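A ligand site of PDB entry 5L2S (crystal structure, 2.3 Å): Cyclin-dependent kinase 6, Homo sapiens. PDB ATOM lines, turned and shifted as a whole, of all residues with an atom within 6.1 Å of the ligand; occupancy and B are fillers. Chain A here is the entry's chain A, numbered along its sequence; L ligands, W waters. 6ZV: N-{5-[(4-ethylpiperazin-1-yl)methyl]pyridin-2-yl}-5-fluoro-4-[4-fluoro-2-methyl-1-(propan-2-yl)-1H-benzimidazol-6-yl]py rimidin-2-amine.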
ATOM      1  N   GLU A  18      11.126  18.890  -2.912  1.00  0.00           N
ATOM      2  CA  GLU A  18      12.428  19.189  -2.330  1.00  0.00           C
ATOM      3  C   GLU A  18      12.824  18.001  -1.451  1.00  0.00           C
ATOM      4  O   GLU A  18      11.995  17.484  -0.703  1.00  0.00           O
ATOM      5  CB  GLU A  18      12.384  20.491  -1.518  1.00  0.00           C
ATOM      6  CG  GLU A  18      13.745  21.110  -1.279  1.00  0.00           C
ATOM      7  CD  GLU A  18      13.744  22.273  -0.293  1.00  0.00           C
ATOM      8  OE1 GLU A  18      13.472  23.411  -0.716  1.00  0.00           O
ATOM      9  OE2 GLU A  18      14.040  22.032   0.900  1.00  0.00           O
ATOM     10  N   ILE A  19      14.094  17.564  -1.578  1.00  0.00           N
ATOM     11  CA  ILE A  19      14.680  16.462  -0.812  1.00  0.00           C
ATOM     12  C   ILE A  19      15.525  17.032   0.341  1.00  0.00           C
ATOM     13  O   ILE A  19      15.511  16.492   1.441  1.00  0.00           O
ATOM     14  CB  ILE A  19      15.486  15.477  -1.733  1.00  0.00           C
ATOM     15  CG1 ILE A  19      14.561  14.758  -2.751  1.00  0.00           C
ATOM     16  CG2 ILE A  19      16.273  14.451  -0.909  1.00  0.00           C
ATOM     17  CD1 ILE A  19      15.314  13.915  -3.834  1.00  0.00           C
ATOM     18  N   GLY A  20      16.267  18.103   0.055  1.00  0.00           N
ATOM     19  CA  GLY A  20      17.132  18.727   1.052  1.00  0.00           C
ATOM     20  C   GLY A  20      17.605  20.115   0.680  1.00  0.00           C
ATOM     21  O   GLY A  20      17.550  20.510  -0.483  1.00  0.00           O
ATOM     22  N   GLU A  21      18.085  20.842   1.702  1.00  0.00           N
ATOM     23  CA  GLU A  21      18.584  22.214   1.594  1.00  0.00           C
ATOM     24  C   GLU A  21      19.667  22.435   2.670  1.00  0.00           C
ATOM     25  O   GLU A  21      19.556  21.913   3.781  1.00  0.00           O
ATOM     26  CB  GLU A  21      17.390  23.211   1.720  1.00  0.00           C
ATOM     27  CG  GLU A  21      17.629  24.525   2.451  1.00  0.00           C
ATOM     28  CD  GLU A  21      18.140  25.679   1.608  1.00  0.00           C
ATOM     29  OE1 GLU A  21      17.416  26.703   1.521  1.00  0.00           O
ATOM     30  OE2 GLU A  21      19.265  25.588   1.080  1.00  0.00           O
ATOM     31  N   TYR A  24      25.304  23.929   0.610  1.00  0.00           N
ATOM     32  CA  TYR A  24      25.665  23.226  -0.628  1.00  0.00           C
ATOM     33  C   TYR A  24      24.705  23.705  -1.717  1.00  0.00           C
ATOM     34  O   TYR A  24      25.082  23.817  -2.880  1.00  0.00           O
ATOM     35  CB  TYR A  24      25.614  21.683  -0.463  1.00  0.00           C
ATOM     36  CG  TYR A  24      24.334  21.124   0.126  1.00  0.00           C
ATOM     37  CD1 TYR A  24      23.271  20.743  -0.693  1.00  0.00           C
ATOM     38  CD2 TYR A  24      24.212  20.896   1.497  1.00  0.00           C
ATOM     39  CE1 TYR A  24      22.094  20.218  -0.149  1.00  0.00           C
ATOM     40  CE2 TYR A  24      23.047  20.369   2.050  1.00  0.00           C
ATOM     41  CZ  TYR A  24      21.978  20.046   1.224  1.00  0.00           C
ATOM     42  OH  TYR A  24      20.840  19.494   1.772  1.00  0.00           O
ATOM     43  N   VAL A  27      18.596  20.059  -3.057  1.00  0.00           N
ATOM     44  CA  VAL A  27      18.434  18.780  -3.729  1.00  0.00           C
ATOM     45  C   VAL A  27      16.938  18.610  -4.006  1.00  0.00           C
ATOM     46  O   VAL A  27      16.137  18.669  -3.079  1.00  0.00           O
ATOM     47  CB  VAL A  27      19.028  17.570  -2.944  1.00  0.00           C
ATOM     48  CG1 VAL A  27      18.848  16.263  -3.713  1.00  0.00           C
ATOM     49  CG2 VAL A  27      20.495  17.786  -2.587  1.00  0.00           C
ATOM     50  N   ALA A  41      17.375  12.812  -8.976  1.00  0.00           N
ATOM     51  CA  ALA A  41      17.669  13.751  -7.921  1.00  0.00           C
ATOM     52  C   ALA A  41      18.592  14.830  -8.495  1.00  0.00           C
ATOM     53  O   ALA A  41      19.671  14.479  -8.974  1.00  0.00           O
ATOM     54  CB  ALA A  41      18.320  13.036  -6.744  1.00  0.00           C
ATOM     55  N   LYS A  43      20.864  18.149  -7.842  1.00  0.00           N
ATOM     56  CA  LYS A  43      21.581  18.916  -6.837  1.00  0.00           C
ATOM     57  C   LYS A  43      22.121  20.190  -7.512  1.00  0.00           C
ATOM     58  O   LYS A  43      22.854  20.102  -8.507  1.00  0.00           O
ATOM     59  CB  LYS A  43      22.697  18.067  -6.206  1.00  0.00           C
ATOM     60  CG  LYS A  43      23.477  18.766  -5.098  1.00  0.00           C
ATOM     61  CD  LYS A  43      24.559  17.874  -4.535  1.00  0.00           C
ATOM     62  CE  LYS A  43      24.759  18.108  -3.056  1.00  0.00           C
ATOM     63  NZ  LYS A  43      25.743  17.160  -2.470  1.00  0.00           N
ATOM     64  N   VAL A  77      25.465   6.043  -5.772  1.00  0.00           N
ATOM     65  CA  VAL A  77      24.387   6.586  -6.596  1.00  0.00           C
ATOM     66  C   VAL A  77      24.918   6.818  -8.038  1.00  0.00           C
ATOM     67  O   VAL A  77      26.089   7.185  -8.198  1.00  0.00           O
ATOM     68  CB  VAL A  77      23.803   7.840  -5.900  1.00  0.00           C
ATOM     69  CG1 VAL A  77      24.735   9.055  -5.966  1.00  0.00           C
ATOM     70  CG2 VAL A  77      22.430   8.171  -6.419  1.00  0.00           C
ATOM     71  N   ARG A  78      24.098   6.499  -9.064  1.00  0.00           N
ATOM     72  CA  ARG A  78      24.477   6.685 -10.482  1.00  0.00           C
ATOM     73  C   ARG A  78      24.479   8.156 -10.759  1.00  0.00           C
ATOM     74  O   ARG A  78      23.596   8.843 -10.252  1.00  0.00           O
ATOM     75  CB  ARG A  78      23.458   6.018 -11.441  1.00  0.00           C
ATOM     76  CG  ARG A  78      23.464   4.488 -11.565  1.00  0.00           C
ATOM     77  CD  ARG A  78      24.677   3.889 -12.292  1.00  0.00           C
ATOM     78  NE  ARG A  78      25.912   4.113 -11.534  1.00  0.00           N
ATOM     79  CZ  ARG A  78      26.241   3.481 -10.405  1.00  0.00           C
ATOM     80  NH1 ARG A  78      25.470   2.521  -9.913  1.00  0.00           N
ATOM     81  NH2 ARG A  78      27.364   3.802  -9.765  1.00  0.00           N
ATOM     82  N   LEU A  96      23.845  18.599 -10.812  1.00  0.00           N
ATOM     83  CA  LEU A  96      24.258  17.200 -10.775  1.00  0.00           C
ATOM     84  C   LEU A  96      23.009  16.331 -10.809  1.00  0.00           C
ATOM     85  O   LEU A  96      22.166  16.428  -9.936  1.00  0.00           O
ATOM     86  CB  LEU A  96      25.063  16.920  -9.488  1.00  0.00           C
ATOM     87  CG  LEU A  96      26.580  16.782  -9.578  1.00  0.00           C
ATOM     88  CD1 LEU A  96      27.204  17.746 -10.586  1.00  0.00           C
ATOM     89  CD2 LEU A  96      27.201  17.003  -8.223  1.00  0.00           C
ATOM     90  N   PHE A  98      21.439  12.720 -10.517  1.00  0.00           N
ATOM     91  CA  PHE A  98      21.678  11.349 -10.046  1.00  0.00           C
ATOM     92  C   PHE A  98      20.437  10.510 -10.189  1.00  0.00           C
ATOM     93  O   PHE A  98      19.355  11.070 -10.257  1.00  0.00           O
ATOM     94  CB  PHE A  98      22.071  11.347  -8.567  1.00  0.00           C
ATOM     95  CG  PHE A  98      23.215  12.240  -8.176  1.00  0.00           C
ATOM     96  CD1 PHE A  98      24.537  11.832  -8.365  1.00  0.00           C
ATOM     97  CD2 PHE A  98      22.988  13.461  -7.548  1.00  0.00           C
ATOM     98  CE1 PHE A  98      25.596  12.653  -7.982  1.00  0.00           C
ATOM     99  CE2 PHE A  98      24.057  14.285  -7.166  1.00  0.00           C
ATOM    100  CZ  PHE A  98      25.349  13.868  -7.375  1.00  0.00           C
ATOM    101  N   GLU A  99      20.584   9.151 -10.128  1.00  0.00           N
ATOM    102  CA  GLU A  99      19.430   8.244 -10.083  1.00  0.00           C
ATOM    103  C   GLU A  99      18.721   8.581  -8.764  1.00  0.00           C
ATOM    104  O   GLU A  99      19.392   8.870  -7.772  1.00  0.00           O
ATOM    105  CB  GLU A  99      19.843   6.755 -10.096  1.00  0.00           C
ATOM    106  CG  GLU A  99      20.581   6.281  -8.861  1.00  0.00           C
ATOM    107  CD  GLU A  99      20.934   4.810  -8.747  1.00  0.00           C
ATOM    108  OE1 GLU A  99      22.124   4.510  -8.484  1.00  0.00           O
ATOM    109  OE2 GLU A  99      20.016   3.966  -8.842  1.00  0.00           O
ATOM    110  N   HIS A 100      17.381   8.576  -8.763  1.00  0.00           N
ATOM    111  CA  HIS A 100      16.639   8.859  -7.539  1.00  0.00           C
ATOM    112  C   HIS A 100      16.468   7.572  -6.750  1.00  0.00           C
ATOM    113  O   HIS A 100      16.277   6.505  -7.336  1.00  0.00           O
ATOM    114  CB  HIS A 100      15.271   9.490  -7.874  1.00  0.00           C
ATOM    115  CG  HIS A 100      14.356   9.631  -6.697  1.00  0.00           C
ATOM    116  ND1 HIS A 100      13.466   8.631  -6.346  1.00  0.00           N
ATOM    117  CD2 HIS A 100      14.270  10.626  -5.781  1.00  0.00           C
ATOM    118  CE1 HIS A 100      12.860   9.050  -5.249  1.00  0.00           C
ATOM    119  NE2 HIS A 100      13.308  10.252  -4.874  1.00  0.00           N
ATOM    120  N   VAL A 101      16.574   7.662  -5.418  1.00  0.00           N
ATOM    121  CA  VAL A 101      16.306   6.534  -4.535  1.00  0.00           C
ATOM    122  C   VAL A 101      15.346   7.048  -3.453  1.00  0.00           C
ATOM    123  O   VAL A 101      15.471   8.190  -3.011  1.00  0.00           O
ATOM    124  CB  VAL A 101      17.520   5.681  -4.041  1.00  0.00           C
ATOM    125  CG1 VAL A 101      18.865   6.253  -4.480  1.00  0.00           C
ATOM    126  CG2 VAL A 101      17.471   5.341  -2.564  1.00  0.00           C
ATOM    127  N   ASP A 102      14.296   6.259  -3.175  1.00  0.00           N
ATOM    128  CA  ASP A 102      13.144   6.595  -2.339  1.00  0.00           C
ATOM    129  C   ASP A 102      13.440   6.973  -0.901  1.00  0.00           C
ATOM    130  O   ASP A 102      12.732   7.830  -0.358  1.00  0.00           O
ATOM    131  CB  ASP A 102      12.092   5.470  -2.381  1.00  0.00           C
ATOM    132  CG  ASP A 102      11.173   5.517  -3.587  1.00  0.00           C
ATOM    133  OD1 ASP A 102      10.494   6.553  -3.774  1.00  0.00           O
ATOM    134  OD2 ASP A 102      11.089   4.495  -4.313  1.00  0.00           O
ATOM    135  N   GLN A 103      14.395   6.314  -0.251  1.00  0.00           N
ATOM    136  CA  GLN A 103      14.649   6.610   1.147  1.00  0.00           C
ATOM    137  C   GLN A 103      16.109   6.614   1.546  1.00  0.00           C
ATOM    138  O   GLN A 103      16.967   6.111   0.803  1.00  0.00           O
ATOM    139  CB  GLN A 103      13.841   5.661   2.057  1.00  0.00           C
ATOM    140  CG  GLN A 103      14.298   4.207   2.064  1.00  0.00           C
ATOM    141  CD  GLN A 103      13.251   3.344   2.695  1.00  0.00           C
ATOM    142  OE1 GLN A 103      13.362   2.931   3.852  1.00  0.00           O
ATOM    143  NE2 GLN A 103      12.185   3.066   1.943  1.00  0.00           N
ATOM    144  N   ASP A 104      16.392   7.169   2.744  1.00  0.00           N
ATOM    145  CA  ASP A 104      17.713   7.188   3.356  1.00  0.00           C
ATOM    146  C   ASP A 104      17.705   6.129   4.483  1.00  0.00           C
ATOM    147  O   ASP A 104      16.669   5.526   4.708  1.00  0.00           O
ATOM    148  CB  ASP A 104      18.078   8.618   3.853  1.00  0.00           C
ATOM    149  CG  ASP A 104      17.212   9.247   4.927  1.00  0.00           C
ATOM    150  OD1 ASP A 104      16.260   8.596   5.393  1.00  0.00           O
ATOM    151  OD2 ASP A 104      17.512  10.386   5.341  1.00  0.00           O
ATOM    152  N   THR A 107      15.172   7.178   7.627  1.00  0.00           N
ATOM    153  CA  THR A 107      13.764   6.794   7.441  1.00  0.00           C
ATOM    154  C   THR A 107      13.613   5.262   7.484  1.00  0.00           C
ATOM    155  O   THR A 107      12.631   4.792   8.077  1.00  0.00           O
ATOM    156  CB  THR A 107      13.128   7.437   6.209  1.00  0.00           C
ATOM    157  OG1 THR A 107      13.920   7.132   5.079  1.00  0.00           O
ATOM    158  CG2 THR A 107      13.007   8.934   6.347  1.00  0.00           C
ATOM    159  N   GLN A 149      21.828   9.881   6.838  1.00  0.00           N
ATOM    160  CA  GLN A 149      21.160  10.833   5.942  1.00  0.00           C
ATOM    161  C   GLN A 149      21.651  10.774   4.501  1.00  0.00           C
ATOM    162  O   GLN A 149      20.916  11.169   3.606  1.00  0.00           O
ATOM    163  CB  GLN A 149      21.226  12.273   6.489  1.00  0.00           C
ATOM    164  CG  GLN A 149      20.246  12.549   7.635  1.00  0.00           C
ATOM    165  CD  GLN A 149      20.694  12.058   9.005  1.00  0.00           C
ATOM    166  OE1 GLN A 149      19.880  11.835   9.900  1.00  0.00           O
ATOM    167  NE2 GLN A 149      22.007  11.879   9.215  1.00  0.00           N
ATOM    168  N   ASN A 150      22.899  10.322   4.250  1.00  0.00           N
ATOM    169  CA  ASN A 150      23.376  10.243   2.868  1.00  0.00           C
ATOM    170  C   ASN A 150      23.751   8.799   2.474  1.00  0.00           C
ATOM    171  O   ASN A 150      24.447   8.573   1.491  1.00  0.00           O
ATOM    172  CB  ASN A 150      24.472  11.291   2.541  1.00  0.00           C
ATOM    173  CG  ASN A 150      25.610  11.360   3.510  1.00  0.00           C
ATOM    174  OD1 ASN A 150      26.113  10.337   3.993  1.00  0.00           O
ATOM    175  ND2 ASN A 150      26.076  12.589   3.763  1.00  0.00           N
ATOM    176  N   LEU A 152      21.705   5.795   1.186  1.00  0.00           N
ATOM    177  CA  LEU A 152      20.363   5.579   0.623  1.00  0.00           C
ATOM    178  C   LEU A 152      20.014   4.106   0.490  1.00  0.00           C
ATOM    179  O   LEU A 152      20.894   3.301   0.186  1.00  0.00           O
ATOM    180  CB  LEU A 152      20.198   6.342  -0.705  1.00  0.00           C
ATOM    181  CG  LEU A 152      20.691   7.794  -0.723  1.00  0.00           C
ATOM    182  CD1 LEU A 152      20.639   8.343  -2.117  1.00  0.00           C
ATOM    183  CD2 LEU A 152      19.911   8.681   0.229  1.00  0.00           C
ATOM    184  N   ALA A 162      25.618   8.531  -1.343  1.00  0.00           N
ATOM    185  CA  ALA A 162      25.402   9.818  -2.008  1.00  0.00           C
ATOM    186  C   ALA A 162      26.207  10.888  -1.270  1.00  0.00           C
ATOM    187  O   ALA A 162      26.810  10.590  -0.236  1.00  0.00           O
ATOM    188  CB  ALA A 162      23.918  10.183  -2.001  1.00  0.00           C
ATOM    189  N   ASP A 163      26.224  12.132  -1.824  1.00  0.00           N
ATOM    190  CA  ASP A 163      26.841  13.346  -1.271  1.00  0.00           C
ATOM    191  C   ASP A 163      28.341  13.214  -0.971  1.00  0.00           C
ATOM    192  O   ASP A 163      28.767  13.355   0.192  1.00  0.00           O
ATOM    193  CB  ASP A 163      26.051  13.826  -0.032  1.00  0.00           C
ATOM    194  CG  ASP A 163      26.508  15.148   0.548  1.00  0.00           C
ATOM    195  OD1 ASP A 163      27.039  15.986  -0.236  1.00  0.00           O
ATOM    196  OD2 ASP A 163      26.379  15.333   1.780  1.00  0.00           O
ATOM    197  N   PHE A 164      29.152  12.973  -2.011  1.00  0.00           N
ATOM    198  CA  PHE A 164      30.610  12.808  -1.927  1.00  0.00           C
ATOM    199  C   PHE A 164      31.256  13.399  -3.165  1.00  0.00           C
ATOM    200  O   PHE A 164      30.580  13.626  -4.153  1.00  0.00           O
ATOM    201  CB  PHE A 164      31.003  11.307  -1.755  1.00  0.00           C
ATOM    202  CG  PHE A 164      30.544  10.397  -2.882  1.00  0.00           C
ATOM    203  CD1 PHE A 164      31.267  10.318  -4.070  1.00  0.00           C
ATOM    204  CD2 PHE A 164      29.399   9.634  -2.754  1.00  0.00           C
ATOM    205  CE1 PHE A 164      30.838   9.502  -5.117  1.00  0.00           C
ATOM    206  CE2 PHE A 164      28.976   8.796  -3.801  1.00  0.00           C
ATOM    207  CZ  PHE A 164      29.693   8.743  -4.976  1.00  0.00           C
HETATM  208  C1  6ZV L   1      13.487  15.393   5.405  1.00  0.00           C
HETATM  209  C2  6ZV L   1      17.904  10.850  -2.920  1.00  0.00           C
HETATM  210  C3  6ZV L   1      13.566  16.882   5.344  1.00  0.00           C
HETATM  211  C4  6ZV L   1      19.949  11.855  -3.266  1.00  0.00           C
HETATM  212  C5  6ZV L   1      20.143  11.007  -4.421  1.00  0.00           C
HETATM  213  C6  6ZV L   1      19.102  10.129  -4.720  1.00  0.00           C
HETATM  214  N2  6ZV L   1      12.631  14.801   4.343  1.00  0.00           N
HETATM  215  C10 6ZV L   1      16.962  11.430   1.409  1.00  0.00           C
HETATM  216  C   6ZV L   1      17.402  11.224   0.111  1.00  0.00           C
HETATM  217  C17 6ZV L   1      20.811  13.407  -1.504  1.00  0.00           C
HETATM  218  C21 6ZV L   1      21.954  13.348  -3.615  1.00  0.00           C
HETATM  219  C12 6ZV L   1      14.749  10.957   0.702  1.00  0.00           C
HETATM  220  C16 6ZV L   1      20.918  12.887  -2.800  1.00  0.00           C
HETATM  221  C11 6ZV L   1      15.614  11.305   1.734  1.00  0.00           C
HETATM  222  C19 6ZV L   1      22.795  14.815  -1.875  1.00  0.00           C
HETATM  223  C18 6ZV L   1      21.737  14.357  -1.078  1.00  0.00           C
HETATM  224  C20 6ZV L   1      22.859  14.263  -3.146  1.00  0.00           C
HETATM  225  C8  6ZV L   1      16.446  10.883  -0.861  1.00  0.00           C
HETATM  226  C23 6ZV L   1      22.971  15.870  -0.016  1.00  0.00           C
HETATM  227  C31 6ZV L   1      13.409  12.471   4.572  1.00  0.00           C
HETATM  228  C35 6ZV L   1      14.442  13.880   2.935  1.00  0.00           C
HETATM  229  C32 6ZV L   1      12.225  13.423   4.655  1.00  0.00           C
HETATM  230  C34 6ZV L   1      13.267  14.842   3.022  1.00  0.00           C
HETATM  231  C25 6ZV L   1      23.442  16.768   1.071  1.00  0.00           C
HETATM  232  C27 6ZV L   1      20.652  13.884   1.960  1.00  0.00           C
HETATM  233  C28 6ZV L   1      19.520  15.714   0.644  1.00  0.00           C
HETATM  234  C14 6ZV L   1      15.126  11.553   3.136  1.00  0.00           C
HETATM  235  C26 6ZV L   1      20.823  15.177   1.206  1.00  0.00           C
HETATM  236  N   6ZV L   1      15.141  10.745  -0.559  1.00  0.00           N
HETATM  237  N1  6ZV L   1      17.980  10.035  -3.987  1.00  0.00           N
HETATM  238  N24 6ZV L   1      23.538  15.757  -1.184  1.00  0.00           N
HETATM  239  N3  6ZV L   1      18.831  11.749  -2.528  1.00  0.00           N
HETATM  240  N22 6ZV L   1      21.861  15.057   0.141  1.00  0.00           N
HETATM  241  N30 6ZV L   1      14.005  12.502   3.230  1.00  0.00           N
HETATM  242  N7  6ZV L   1      16.737  10.725  -2.215  1.00  0.00           N
HETATM  243  F29 6ZV L   1      23.888  14.635  -3.943  1.00  0.00           F
HETATM  244  F15 6ZV L   1      21.284  10.944  -5.147  1.00  0.00           F
HETATM  245  O   HOH W   1      13.104  11.281  -2.397  1.00  0.00           O
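NZ of Lys 43 lies within hydrogen-bond range of N24 of the ligand, 2.9 Å away. The backbone NH (N) of Val 101 is in hydrogen-bond range of a nitrogen (N1) of the ligand, 3.1 Å away. The backbone carbonyl oxygen (O) of Val 101 sits close to a nitrogen (N7) of the ligand, 2.9 Å away.
Merely in contact with the ligand: Ile 19 (3.2 Å), Gly 20 (3.9 Å), Tyr 24 (3.6 Å), Val 27 (3.8 Å), Ala 41 (3.6 Å), Val 77 (3.3 Å), Phe 98 (3.2 Å), Glu 99 (3.3 Å), His 100 (3.95 Å), Asp 102 (3.8 Å), Asp 104 (3.5 Å), Thr 107 (3.98 Å), Gln 149 (3.2 Å), Leu 152 (3.5 Å) and Asp 163 (3.3 Å). Hydrophobic or aromatic side chains that line the ligand: Ile 19, Tyr 24, Val 27, Ala 41, Val 77, Phe 98, Val 101 and Leu 152. Within 4 Å of the ligand: Ile 19, Gly 20, Tyr 24, Val 27, Ala 41, Lys 43, Val 77, Phe 98, Glu 99, His 100, Val 101, Asp 102, Asp 104, Thr 107, Gln 149, Leu 152 and Asp 163.
The side-chain carboxylate (OD1) of Asp 104 is in hydrogen-bond range of the side-chain hydroxyl (OG1) of Thr 107, 2.8 Å away. The backbone carbonyl oxygen of Lys 43 is in hydrogen-bond range of the backbone NH of Leu 96, at 2.9 Å. The backbone NH (N) of Arg 78 sits at hydrogen-bond distance from the side-chain carboxylate (OE1) of Glu 99, at 2.9 Å. The backbone NH (N) of Phe 98 sits at hydrogen-bond distance from the backbone carbonyl oxygen (O) of Ala 41. The backbone NH (N) of Glu 21 sits at hydrogen-bond distance from the side-chain hydroxyl (OH) of Tyr 24. The backbone NH (N) of Val 27 lies within hydrogen-bond range of the backbone carbonyl oxygen (O) of Gly 20, 2.8 Å away. O of Val 27 sits at hydrogen-bond distance from N of Ile 19, at 2.8 Å. OD2 of Asp 163 sits at hydrogen-bond distance from ND2 of Asn 150, at 3.4 Å.
Water W1 lies within hydrogen-bond range of NE2 of His 100 (2.7 Å) and N of the ligand (2.8 Å).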
